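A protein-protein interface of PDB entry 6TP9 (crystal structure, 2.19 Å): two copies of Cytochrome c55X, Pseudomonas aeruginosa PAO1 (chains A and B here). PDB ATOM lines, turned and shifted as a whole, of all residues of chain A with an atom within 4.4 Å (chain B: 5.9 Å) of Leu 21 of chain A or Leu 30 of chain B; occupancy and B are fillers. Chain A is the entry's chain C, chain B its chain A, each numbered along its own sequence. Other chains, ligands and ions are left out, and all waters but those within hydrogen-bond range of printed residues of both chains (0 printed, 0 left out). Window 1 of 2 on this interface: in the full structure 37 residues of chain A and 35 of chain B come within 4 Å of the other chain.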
ATOM      1  N   ARG A  17      -3.379  30.488   6.602  1.00  0.00           N
ATOM      2  CA  ARG A  17      -2.901  29.501   5.638  1.00  0.00           C
ATOM      3  C   ARG A  17      -1.402  29.636   5.430  1.00  0.00           C
ATOM      4  O   ARG A  17      -0.686  28.633   5.332  1.00  0.00           O
ATOM      5  CB  ARG A  17      -3.630  29.649   4.305  1.00  0.00           C
ATOM      6  CG  ARG A  17      -5.082  29.260   4.373  1.00  0.00           C
ATOM      7  CD  ARG A  17      -5.682  29.053   2.999  1.00  0.00           C
ATOM      8  NE  ARG A  17      -7.129  28.913   3.103  1.00  0.00           N
ATOM      9  CZ  ARG A  17      -7.745  27.808   3.503  1.00  0.00           C
ATOM     10  NH1 ARG A  17      -7.043  26.732   3.833  1.00  0.00           N
ATOM     11  NH2 ARG A  17      -9.069  27.778   3.574  1.00  0.00           N
ATOM     12  N   HIS A  18      -0.906  30.871   5.362  1.00  0.00           N
ATOM     13  CA  HIS A  18       0.529  31.075   5.228  1.00  0.00           C
ATOM     14  C   HIS A  18       1.274  30.432   6.391  1.00  0.00           C
ATOM     15  O   HIS A  18       2.223  29.665   6.189  1.00  0.00           O
ATOM     16  CB  HIS A  18       0.841  32.568   5.147  1.00  0.00           C
ATOM     17  CG  HIS A  18       2.277  32.863   4.859  1.00  0.00           C
ATOM     18  ND1 HIS A  18       2.791  32.882   3.580  1.00  0.00           N
ATOM     19  CD2 HIS A  18       3.315  33.133   5.686  1.00  0.00           C
ATOM     20  CE1 HIS A  18       4.081  33.162   3.631  1.00  0.00           C
ATOM     21  NE2 HIS A  18       4.424  33.319   4.897  1.00  0.00           N
ATOM     22  N   LEU A  19       0.849  30.727   7.622  1.00  0.00           N
ATOM     23  CA  LEU A  19       1.470  30.109   8.787  1.00  0.00           C
ATOM     24  C   LEU A  19       1.455  28.592   8.667  1.00  0.00           C
ATOM     25  O   LEU A  19       2.451  27.922   8.965  1.00  0.00           O
ATOM     26  CB  LEU A  19       0.743  30.547  10.059  1.00  0.00           C
ATOM     27  CG  LEU A  19       1.317  30.002  11.367  1.00  0.00           C
ATOM     28  CD1 LEU A  19       2.669  30.640  11.649  1.00  0.00           C
ATOM     29  CD2 LEU A  19       0.359  30.234  12.519  1.00  0.00           C
ATOM     30  N   LEU A  20       0.323  28.038   8.232  1.00  0.00           N
ATOM     31  CA  LEU A  20       0.209  26.596   8.051  1.00  0.00           C
ATOM     32  C   LEU A  20       1.284  26.070   7.110  1.00  0.00           C
ATOM     33  O   LEU A  20       1.883  25.018   7.361  1.00  0.00           O
ATOM     34  CB  LEU A  20      -1.178  26.269   7.507  1.00  0.00           C
ATOM     35  CG  LEU A  20      -1.973  25.115   8.107  1.00  0.00           C
ATOM     36  CD1 LEU A  20      -2.067  25.240   9.612  1.00  0.00           C
ATOM     37  CD2 LEU A  20      -3.354  25.117   7.470  1.00  0.00           C
ATOM     38  N   LEU A  21       1.547  26.793   6.021  1.00  0.00           N
ATOM     39  CA  LEU A  21       2.443  26.291   4.989  1.00  0.00           C
ATOM     40  C   LEU A  21       3.908  26.499   5.353  1.00  0.00           C
ATOM     41  O   LEU A  21       4.744  25.629   5.083  1.00  0.00           O
ATOM     42  CB  LEU A  21       2.129  26.976   3.659  1.00  0.00           C
ATOM     43  CG  LEU A  21       0.713  26.772   3.123  1.00  0.00           C
ATOM     44  CD1 LEU A  21       0.520  27.598   1.865  1.00  0.00           C
ATOM     45  CD2 LEU A  21       0.442  25.303   2.857  1.00  0.00           C
ATOM     46  N   GLN A  22       4.240  27.637   5.959  1.00  0.00           N
ATOM     47  CA  GLN A  22       5.633  27.961   6.238  1.00  0.00           C
ATOM     48  C   GLN A  22       6.099  27.427   7.588  1.00  0.00           C
ATOM     49  O   GLN A  22       7.125  26.745   7.667  1.00  0.00           O
ATOM     50  CB  GLN A  22       5.839  29.477   6.174  1.00  0.00           C
ATOM     51  CG  GLN A  22       7.246  29.906   6.537  1.00  0.00           C
ATOM     52  CD  GLN A  22       7.541  31.340   6.153  1.00  0.00           C
ATOM     53  OE1 GLN A  22       6.729  32.005   5.508  1.00  0.00           O
ATOM     54  NE2 GLN A  22       8.714  31.825   6.546  1.00  0.00           N
ATOM     55  N   ASP A  23       5.368  27.728   8.660  1.00  0.00           N
ATOM     56  CA  ASP A  23       5.810  27.354  10.000  1.00  0.00           C
ATOM     57  C   ASP A  23       5.394  25.929  10.357  1.00  0.00           C
ATOM     58  O   ASP A  23       6.247  25.076  10.622  1.00  0.00           O
ATOM     59  CB  ASP A  23       5.267  28.353  11.027  1.00  0.00           C
ATOM     60  CG  ASP A  23       5.831  29.746  10.835  1.00  0.00           C
ATOM     61  OD1 ASP A  23       5.326  30.476   9.956  1.00  0.00           O
ATOM     62  OD2 ASP A  23       6.785  30.108  11.556  1.00  0.00           O
ATOM     63  N   GLY A  25       4.271  23.643   8.447  1.00  0.00           N
ATOM     64  CA  GLY A  25       4.758  22.700   7.456  1.00  0.00           C
ATOM     65  C   GLY A  25       6.228  22.374   7.606  1.00  0.00           C
ATOM     66  O   GLY A  25       6.673  21.300   7.191  1.00  0.00           O
ATOM     67  N   LEU A  30       5.058  18.883   4.217  1.00  0.00           N
ATOM     68  CA  LEU A  30       4.004  19.134   3.242  1.00  0.00           C
ATOM     69  C   LEU A  30       4.066  18.068   2.157  1.00  0.00           C
ATOM     70  O   LEU A  30       5.140  17.801   1.606  1.00  0.00           O
ATOM     71  CB  LEU A  30       4.138  20.523   2.607  1.00  0.00           C
ATOM     72  CG  LEU A  30       3.888  21.742   3.494  1.00  0.00           C
ATOM     73  CD1 LEU A  30       4.155  23.008   2.701  1.00  0.00           C
ATOM     74  CD2 LEU A  30       2.473  21.747   4.043  1.00  0.00           C
ATOM     75  N   ARG A  31       2.917  17.474   1.841  1.00  0.00           N
ATOM     76  CA  ARG A  31       2.831  16.463   0.801  1.00  0.00           C
ATOM     77  C   ARG A  31       1.503  16.587   0.073  1.00  0.00           C
ATOM     78  O   ARG A  31       0.481  16.921   0.678  1.00  0.00           O
ATOM     79  CB  ARG A  31       2.976  15.047   1.376  1.00  0.00           C
ATOM     80  CG  ARG A  31       4.415  14.571   1.458  1.00  0.00           C
ATOM     81  CD  ARG A  31       4.550  13.284   2.255  1.00  0.00           C
ATOM     82  NE  ARG A  31       4.180  12.092   1.495  1.00  0.00           N
ATOM     83  CZ  ARG A  31       4.953  11.514   0.577  1.00  0.00           C
ATOM     84  NH1 ARG A  31       6.141  12.027   0.280  1.00  0.00           N
ATOM     85  NH2 ARG A  31       4.533  10.426  -0.051  1.00  0.00           N
ATOM     86  N   LEU A  32       1.535  16.316  -1.232  1.00  0.00           N
ATOM     87  CA  LEU A  32       0.339  16.296  -2.068  1.00  0.00           C
ATOM     88  C   LEU A  32      -0.121  14.845  -2.168  1.00  0.00           C
ATOM     89  O   LEU A  32       0.200  14.124  -3.107  1.00  0.00           O
ATOM     90  CB  LEU A  32       0.644  16.892  -3.437  1.00  0.00           C
ATOM     91  CG  LEU A  32       1.006  18.376  -3.390  1.00  0.00           C
ATOM     92  CD1 LEU A  32       1.761  18.797  -4.633  1.00  0.00           C
ATOM     93  CD2 LEU A  32      -0.257  19.202  -3.223  1.00  0.00           C
ATOM     94  N   ILE A  90       8.377  20.795  -2.173  1.00  0.00           N
ATOM     95  CA  ILE A  90       7.277  21.714  -2.449  1.00  0.00           C
ATOM     96  C   ILE A  90       7.112  22.770  -1.367  1.00  0.00           C
ATOM     97  O   ILE A  90       6.243  23.645  -1.496  1.00  0.00           O
ATOM     98  CB  ILE A  90       5.940  20.966  -2.635  1.00  0.00           C
ATOM     99  CG1 ILE A  90       5.594  20.154  -1.386  1.00  0.00           C
ATOM    100  CG2 ILE A  90       5.997  20.066  -3.858  1.00  0.00           C
ATOM    101  CD1 ILE A  90       4.124  19.825  -1.281  1.00  0.00           C
ATOM    102  N   PRO A  92       7.184  26.087   0.621  1.00  0.00           N
ATOM    103  CA  PRO A  92       7.395  27.443   0.103  1.00  0.00           C
ATOM    104  C   PRO A  92       8.727  28.025   0.566  1.00  0.00           C
ATOM    105  O   PRO A  92       9.324  28.860  -0.113  1.00  0.00           O
ATOM    106  CB  PRO A  92       6.214  28.228   0.678  1.00  0.00           C
ATOM    107  CG  PRO A  92       5.832  27.493   1.909  1.00  0.00           C
ATOM    108  CD  PRO A  92       6.120  26.041   1.640  1.00  0.00           C
ATOM    109  OXT PRO A  92       9.239  27.663   1.626  1.00  0.00           O
ATOM    110  N   HIS B  18       3.423  29.154  -4.551  1.00  0.00           N
ATOM    111  CA  HIS B  18       2.124  29.508  -3.989  1.00  0.00           C
ATOM    112  C   HIS B  18       1.001  28.835  -4.765  1.00  0.00           C
ATOM    113  O   HIS B  18       0.107  28.214  -4.179  1.00  0.00           O
ATOM    114  CB  HIS B  18       1.944  31.024  -3.989  1.00  0.00           C
ATOM    115  CG  HIS B  18       0.752  31.483  -3.213  1.00  0.00           C
ATOM    116  ND1 HIS B  18      -0.171  32.372  -3.720  1.00  0.00           N
ATOM    117  CD2 HIS B  18       0.323  31.163  -1.969  1.00  0.00           C
ATOM    118  CE1 HIS B  18      -1.115  32.585  -2.820  1.00  0.00           C
ATOM    119  NE2 HIS B  18      -0.839  31.862  -1.749  1.00  0.00           N
ATOM    120  N   LEU B  20       1.085  26.139  -6.530  1.00  0.00           N
ATOM    121  CA  LEU B  20       1.085  24.706  -6.259  1.00  0.00           C
ATOM    122  C   LEU B  20       0.395  24.397  -4.938  1.00  0.00           C
ATOM    123  O   LEU B  20      -0.414  23.463  -4.849  1.00  0.00           O
ATOM    124  CB  LEU B  20       2.522  24.180  -6.240  1.00  0.00           C
ATOM    125  CG  LEU B  20       2.686  22.683  -5.971  1.00  0.00           C
ATOM    126  CD1 LEU B  20       2.069  21.861  -7.086  1.00  0.00           C
ATOM    127  CD2 LEU B  20       4.157  22.332  -5.800  1.00  0.00           C
ATOM    128  N   LEU B  21       0.695  25.173  -3.901  1.00  0.00           N
ATOM    129  CA  LEU B  21       0.245  24.822  -2.563  1.00  0.00           C
ATOM    130  C   LEU B  21      -1.222  25.170  -2.342  1.00  0.00           C
ATOM    131  O   LEU B  21      -1.938  24.418  -1.672  1.00  0.00           O
ATOM    132  CB  LEU B  21       1.132  25.512  -1.528  1.00  0.00           C
ATOM    133  CG  LEU B  21       2.590  25.048  -1.603  1.00  0.00           C
ATOM    134  CD1 LEU B  21       3.490  25.866  -0.699  1.00  0.00           C
ATOM    135  CD2 LEU B  21       2.687  23.569  -1.251  1.00  0.00           C
ATOM    136  N   GLN B  22      -1.697  26.286  -2.895  1.00  0.00           N
ATOM    137  CA  GLN B  22      -3.042  26.754  -2.580  1.00  0.00           C
ATOM    138  C   GLN B  22      -4.061  26.514  -3.685  1.00  0.00           C
ATOM    139  O   GLN B  22      -5.251  26.389  -3.384  1.00  0.00           O
ATOM    140  CB  GLN B  22      -3.013  28.246  -2.225  1.00  0.00           C
ATOM    141  CG  GLN B  22      -2.381  28.511  -0.859  1.00  0.00           C
ATOM    142  CD  GLN B  22      -2.742  29.864  -0.279  1.00  0.00           C
ATOM    143  OE1 GLN B  22      -3.740  30.477  -0.662  1.00  0.00           O
ATOM    144  NE2 GLN B  22      -1.927  30.337   0.658  1.00  0.00           N
ATOM    145  N   GLY B  25      -3.069  22.262  -4.802  1.00  0.00           N
ATOM    146  CA  GLY B  25      -3.183  21.409  -3.633  1.00  0.00           C
ATOM    147  C   GLY B  25      -4.604  21.073  -3.232  1.00  0.00           C
ATOM    148  O   GLY B  25      -4.815  20.084  -2.521  1.00  0.00           O
ATOM    149  N   SER B  26      -5.582  21.871  -3.658  1.00  0.00           N
ATOM    150  CA  SER B  26      -6.972  21.567  -3.331  1.00  0.00           C
ATOM    151  C   SER B  26      -7.378  20.216  -3.910  1.00  0.00           C
ATOM    152  O   SER B  26      -7.723  19.284  -3.174  1.00  0.00           O
ATOM    153  CB  SER B  26      -7.888  22.675  -3.850  1.00  0.00           C
ATOM    154  OG  SER B  26      -7.904  22.704  -5.267  1.00  0.00           O
ATOM    155  N   HIS B  28      -5.433  18.042  -5.546  1.00  0.00           N
ATOM    156  CA  HIS B  28      -4.389  17.043  -5.363  1.00  0.00           C
ATOM    157  C   HIS B  28      -4.054  16.796  -3.896  1.00  0.00           C
ATOM    158  O   HIS B  28      -3.046  16.146  -3.603  1.00  0.00           O
ATOM    159  CB  HIS B  28      -3.133  17.455  -6.137  1.00  0.00           C
ATOM    160  CG  HIS B  28      -3.275  17.338  -7.624  1.00  0.00           C
ATOM    161  ND1 HIS B  28      -3.123  16.143  -8.295  1.00  0.00           N
ATOM    162  CD2 HIS B  28      -3.559  18.265  -8.570  1.00  0.00           C
ATOM    163  CE1 HIS B  28      -3.304  16.339  -9.589  1.00  0.00           C
ATOM    164  NE2 HIS B  28      -3.570  17.618  -9.783  1.00  0.00           N
ATOM    165  N   GLY B  29      -4.869  17.301  -2.976  1.00  0.00           N
ATOM    166  CA  GLY B  29      -4.807  16.881  -1.591  1.00  0.00           C
ATOM    167  C   GLY B  29      -3.555  17.266  -0.833  1.00  0.00           C
ATOM    168  O   GLY B  29      -2.824  16.391  -0.359  1.00  0.00           O
ATOM    169  N   LEU B  30      -3.298  18.563  -0.695  1.00  0.00           N
ATOM    170  CA  LEU B  30      -2.202  19.010   0.153  1.00  0.00           C
ATOM    171  C   LEU B  30      -2.493  18.655   1.608  1.00  0.00           C
ATOM    172  O   LEU B  30      -3.610  18.846   2.100  1.00  0.00           O
ATOM    173  CB  LEU B  30      -1.988  20.515   0.010  1.00  0.00           C
ATOM    174  CG  LEU B  30      -0.799  21.090   0.786  1.00  0.00           C
ATOM    175  CD1 LEU B  30       0.526  20.560   0.255  1.00  0.00           C
ATOM    176  CD2 LEU B  30      -0.820  22.608   0.738  1.00  0.00           C
ATOM    177  N   ARG B  31      -1.480  18.126   2.289  1.00  0.00           N
ATOM    178  CA  ARG B  31      -1.597  17.713   3.678  1.00  0.00           C
ATOM    179  C   ARG B  31      -0.304  18.056   4.400  1.00  0.00           C
ATOM    180  O   ARG B  31       0.760  18.167   3.786  1.00  0.00           O
ATOM    181  CB  ARG B  31      -1.870  16.208   3.812  1.00  0.00           C
ATOM    182  CG  ARG B  31      -3.167  15.731   3.189  1.00  0.00           C
ATOM    183  CD  ARG B  31      -4.380  16.181   3.991  1.00  0.00           C
ATOM    184  NE  ARG B  31      -5.375  16.819   3.133  1.00  0.00           N
ATOM    185  CZ  ARG B  31      -6.383  16.188   2.539  1.00  0.00           C
ATOM    186  NH1 ARG B  31      -6.560  14.885   2.705  1.00  0.00           N
ATOM    187  NH2 ARG B  31      -7.225  16.869   1.775  1.00  0.00           N
ATOM    188  N   LEU B  32      -0.400  18.218   5.719  1.00  0.00           N
ATOM    189  CA  LEU B  32       0.785  18.418   6.554  1.00  0.00           C
ATOM    190  C   LEU B  32       1.216  17.057   7.082  1.00  0.00           C
ATOM    191  O   LEU B  32       0.741  16.584   8.116  1.00  0.00           O
ATOM    192  CB  LEU B  32       0.508  19.401   7.683  1.00  0.00           C
ATOM    193  CG  LEU B  32       0.740  20.871   7.331  1.00  0.00           C
ATOM    194  CD1 LEU B  32      -0.341  21.378   6.392  1.00  0.00           C
ATOM    195  CD2 LEU B  32       0.805  21.719   8.593  1.00  0.00           C
ATOM    196  N   GLY B  88      -9.133  18.333   5.887  1.00  0.00           N
ATOM    197  CA  GLY B  88      -8.320  18.261   4.683  1.00  0.00           C
ATOM    198  C   GLY B  88      -8.436  19.479   3.795  1.00  0.00           C
ATOM    199  O   GLY B  88      -8.553  19.345   2.571  1.00  0.00           O
ATOM    200  N   GLU B  89      -8.392  20.672   4.384  1.00  0.00           N
ATOM    201  CA  GLU B  89      -8.591  21.926   3.666  1.00  0.00           C
ATOM    202  C   GLU B  89      -7.431  22.882   3.911  1.00  0.00           C
ATOM    203  O   GLU B  89      -7.610  24.039   4.296  1.00  0.00           O
ATOM    204  CB  GLU B  89      -9.915  22.564   4.076  1.00  0.00           C
ATOM    205  CG  GLU B  89     -11.092  22.144   3.223  1.00  0.00           C
ATOM    206  CD  GLU B  89     -12.427  22.459   3.871  1.00  0.00           C
ATOM    207  OE1 GLU B  89     -13.467  22.231   3.218  1.00  0.00           O
ATOM    208  OE2 GLU B  89     -12.436  22.928   5.030  1.00  0.00           O
ATOM    209  N   ILE B  90      -6.208  22.409   3.678  1.00  0.00           N
ATOM    210  CA  ILE B  90      -5.059  23.303   3.771  1.00  0.00           C
ATOM    211  C   ILE B  90      -4.987  24.200   2.543  1.00  0.00           C
ATOM    212  O   ILE B  90      -4.681  25.392   2.649  1.00  0.00           O
ATOM    213  CB  ILE B  90      -3.771  22.489   3.973  1.00  0.00           C
ATOM    214  CG1 ILE B  90      -3.793  21.848   5.359  1.00  0.00           C
ATOM    215  CG2 ILE B  90      -2.542  23.371   3.835  1.00  0.00           C
ATOM    216  CD1 ILE B  90      -3.628  20.365   5.338  1.00  0.00           C
ATOM    217  N   ALA B  91      -5.266  23.648   1.369  1.00  0.00           N
ATOM    218  CA  ALA B  91      -5.539  24.492   0.216  1.00  0.00           C
ATOM    219  C   ALA B  91      -6.989  24.970   0.278  1.00  0.00           C
ATOM    220  O   ALA B  91      -7.880  24.194   0.636  1.00  0.00           O
ATOM    221  CB  ALA B  91      -5.296  23.730  -1.081  1.00  0.00           C
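Of chain B, only Gln 22 (3.9 Å), Leu 30 (3.7 Å) and Ile 90 (3.7 Å) come within 4 Å of Leu 21 of chain A. Printed residues of chain A within 4 Å of Leu 20 of chain B: Leu 32 and Ile 90. Of the printed residues of chain A, Gly 25 of chain B touches Leu 32 (3.7 Å). Of the printed residues of chain A, Leu 30 of chain B touches Leu 21, Arg 31, Leu 32 and Ile 90. Of the printed residues of chain A, Leu 32 of chain B touches Leu 20, Gly 25 and Leu 30. Gly 88 of chain B touches none of the printed residues of chain A. The nearest residue of chain B that does not touch Leu 21 of chain A is Leu 21 of chain B (4.03 Å). The nearest printed residue of chain B that does not touch Arg 17 of chain A is Gln 22 of chain B (4.1 Å).
The guanidinium group (NH1) of Arg 17 of chain A lies within hydrogen-bond range of the backbone carbonyl oxygen (O) of Ile 90 of chain B. O of Glu 89 of chain B lies within hydrogen-bond range of NH1 of Arg 17 of chain A, at 2.8 Å. The backbone NH of Arg 31 of chain B sits at hydrogen-bond distance from the backbone carbonyl oxygen of Arg 31 of chain A (2.8 Å).
Hydrophobic or aromatic side chains of chain A that line the printed part of chain B: Leu 20, Leu 21, Leu 30, Leu 32, Ile 90 and Pro 92. Of the 15 printed residues of chain B, 12 touch a printed residue of chain A. Hydrophobic or aromatic side chains of chain B within 4 Å of the printed part of chain A: Leu 20, Leu 21, Leu 30, Leu 32 and Ile 90. Along chain B the printed residues that touch a printed residue of chain A span positions 20 to 91. Among the printed residues, 23 pairs touch across the chains. Among the printed residues, no Asp or Glu carboxylate lies within 4 Å of a Lys or Arg side-chain nitrogen of the other chain.
Leu 20 of chain A touches Leu 32 of chain B, and with the chains exchanged Leu 32 of chain A touches Leu 20 of chain B. Leu 21 of chain A touches Gln 22 of chain B, but with the chains exchanged Gln 22 of chain A does not touch Leu 21 of chain B (6.9 Å). Leu 21 of chain A touches Leu 30 of chain B, but with the chains exchanged Leu 30 of chain A does not touch Leu 21 of chain B (4.3 Å). Ile 90 of chain A touches Leu 30 of chain B, but with the chains exchanged Leu 30 of chain A does not touch Ile 90 of chain B (5.3 Å). Positions printed for both chains: 18, 20, 21, 22, 25, 30, 31, 32 and 90.
A ring nitrogen (NE2) of His 18 of chain B is in hydrogen-bond range of the side-chain amide nitrogen (NE2) of Gln 22 of chain B (3.1 Å). The backbone carbonyl oxygen of Leu 20 of chain A lies within hydrogen-bond range of the backbone NH of Gly 25 of chain A (3.0 Å). NH2 of Arg 31 of chain B lies within hydrogen-bond range of O of Gly 88 of chain B. O of Leu 20 of chain B sits at hydrogen-bond distance from N of Gly 25 of chain B. The backbone NH (N) of Leu 30 of chain B sits at hydrogen-bond distance from the backbone carbonyl oxygen (O) of Gly 25 of chain B, 2.8 Å away.
Arg 17 of chain A touches Ala 91 of chain B. Leu 32 of chain B touches Leu 20 of chain A (CD2 to O, 3.7 Å). CD2 of Leu 20 of chain A touches CG1 of Ile 90 of chain B (3.9 Å). CD2 of Leu 21 of chain A touches CD2 of Leu 30 of chain B (3.7 Å). Leu 32 of chain B touches Gly 25 of chain A. CA of Leu 30 of chain A touches O of Arg 31 of chain B, at 3.4 Å. Arg 31 of chain A touches Gly 29 of chain B. CD2 of Leu 32 of chain A touches CA of Gly 25 of chain B, at 3.7 Å. Ile 90 of chain A touches Leu 21 of chain B. Leu 30 of chain B touches Ile 90 of chain A (CD1 to CD1, 3.98 Å).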
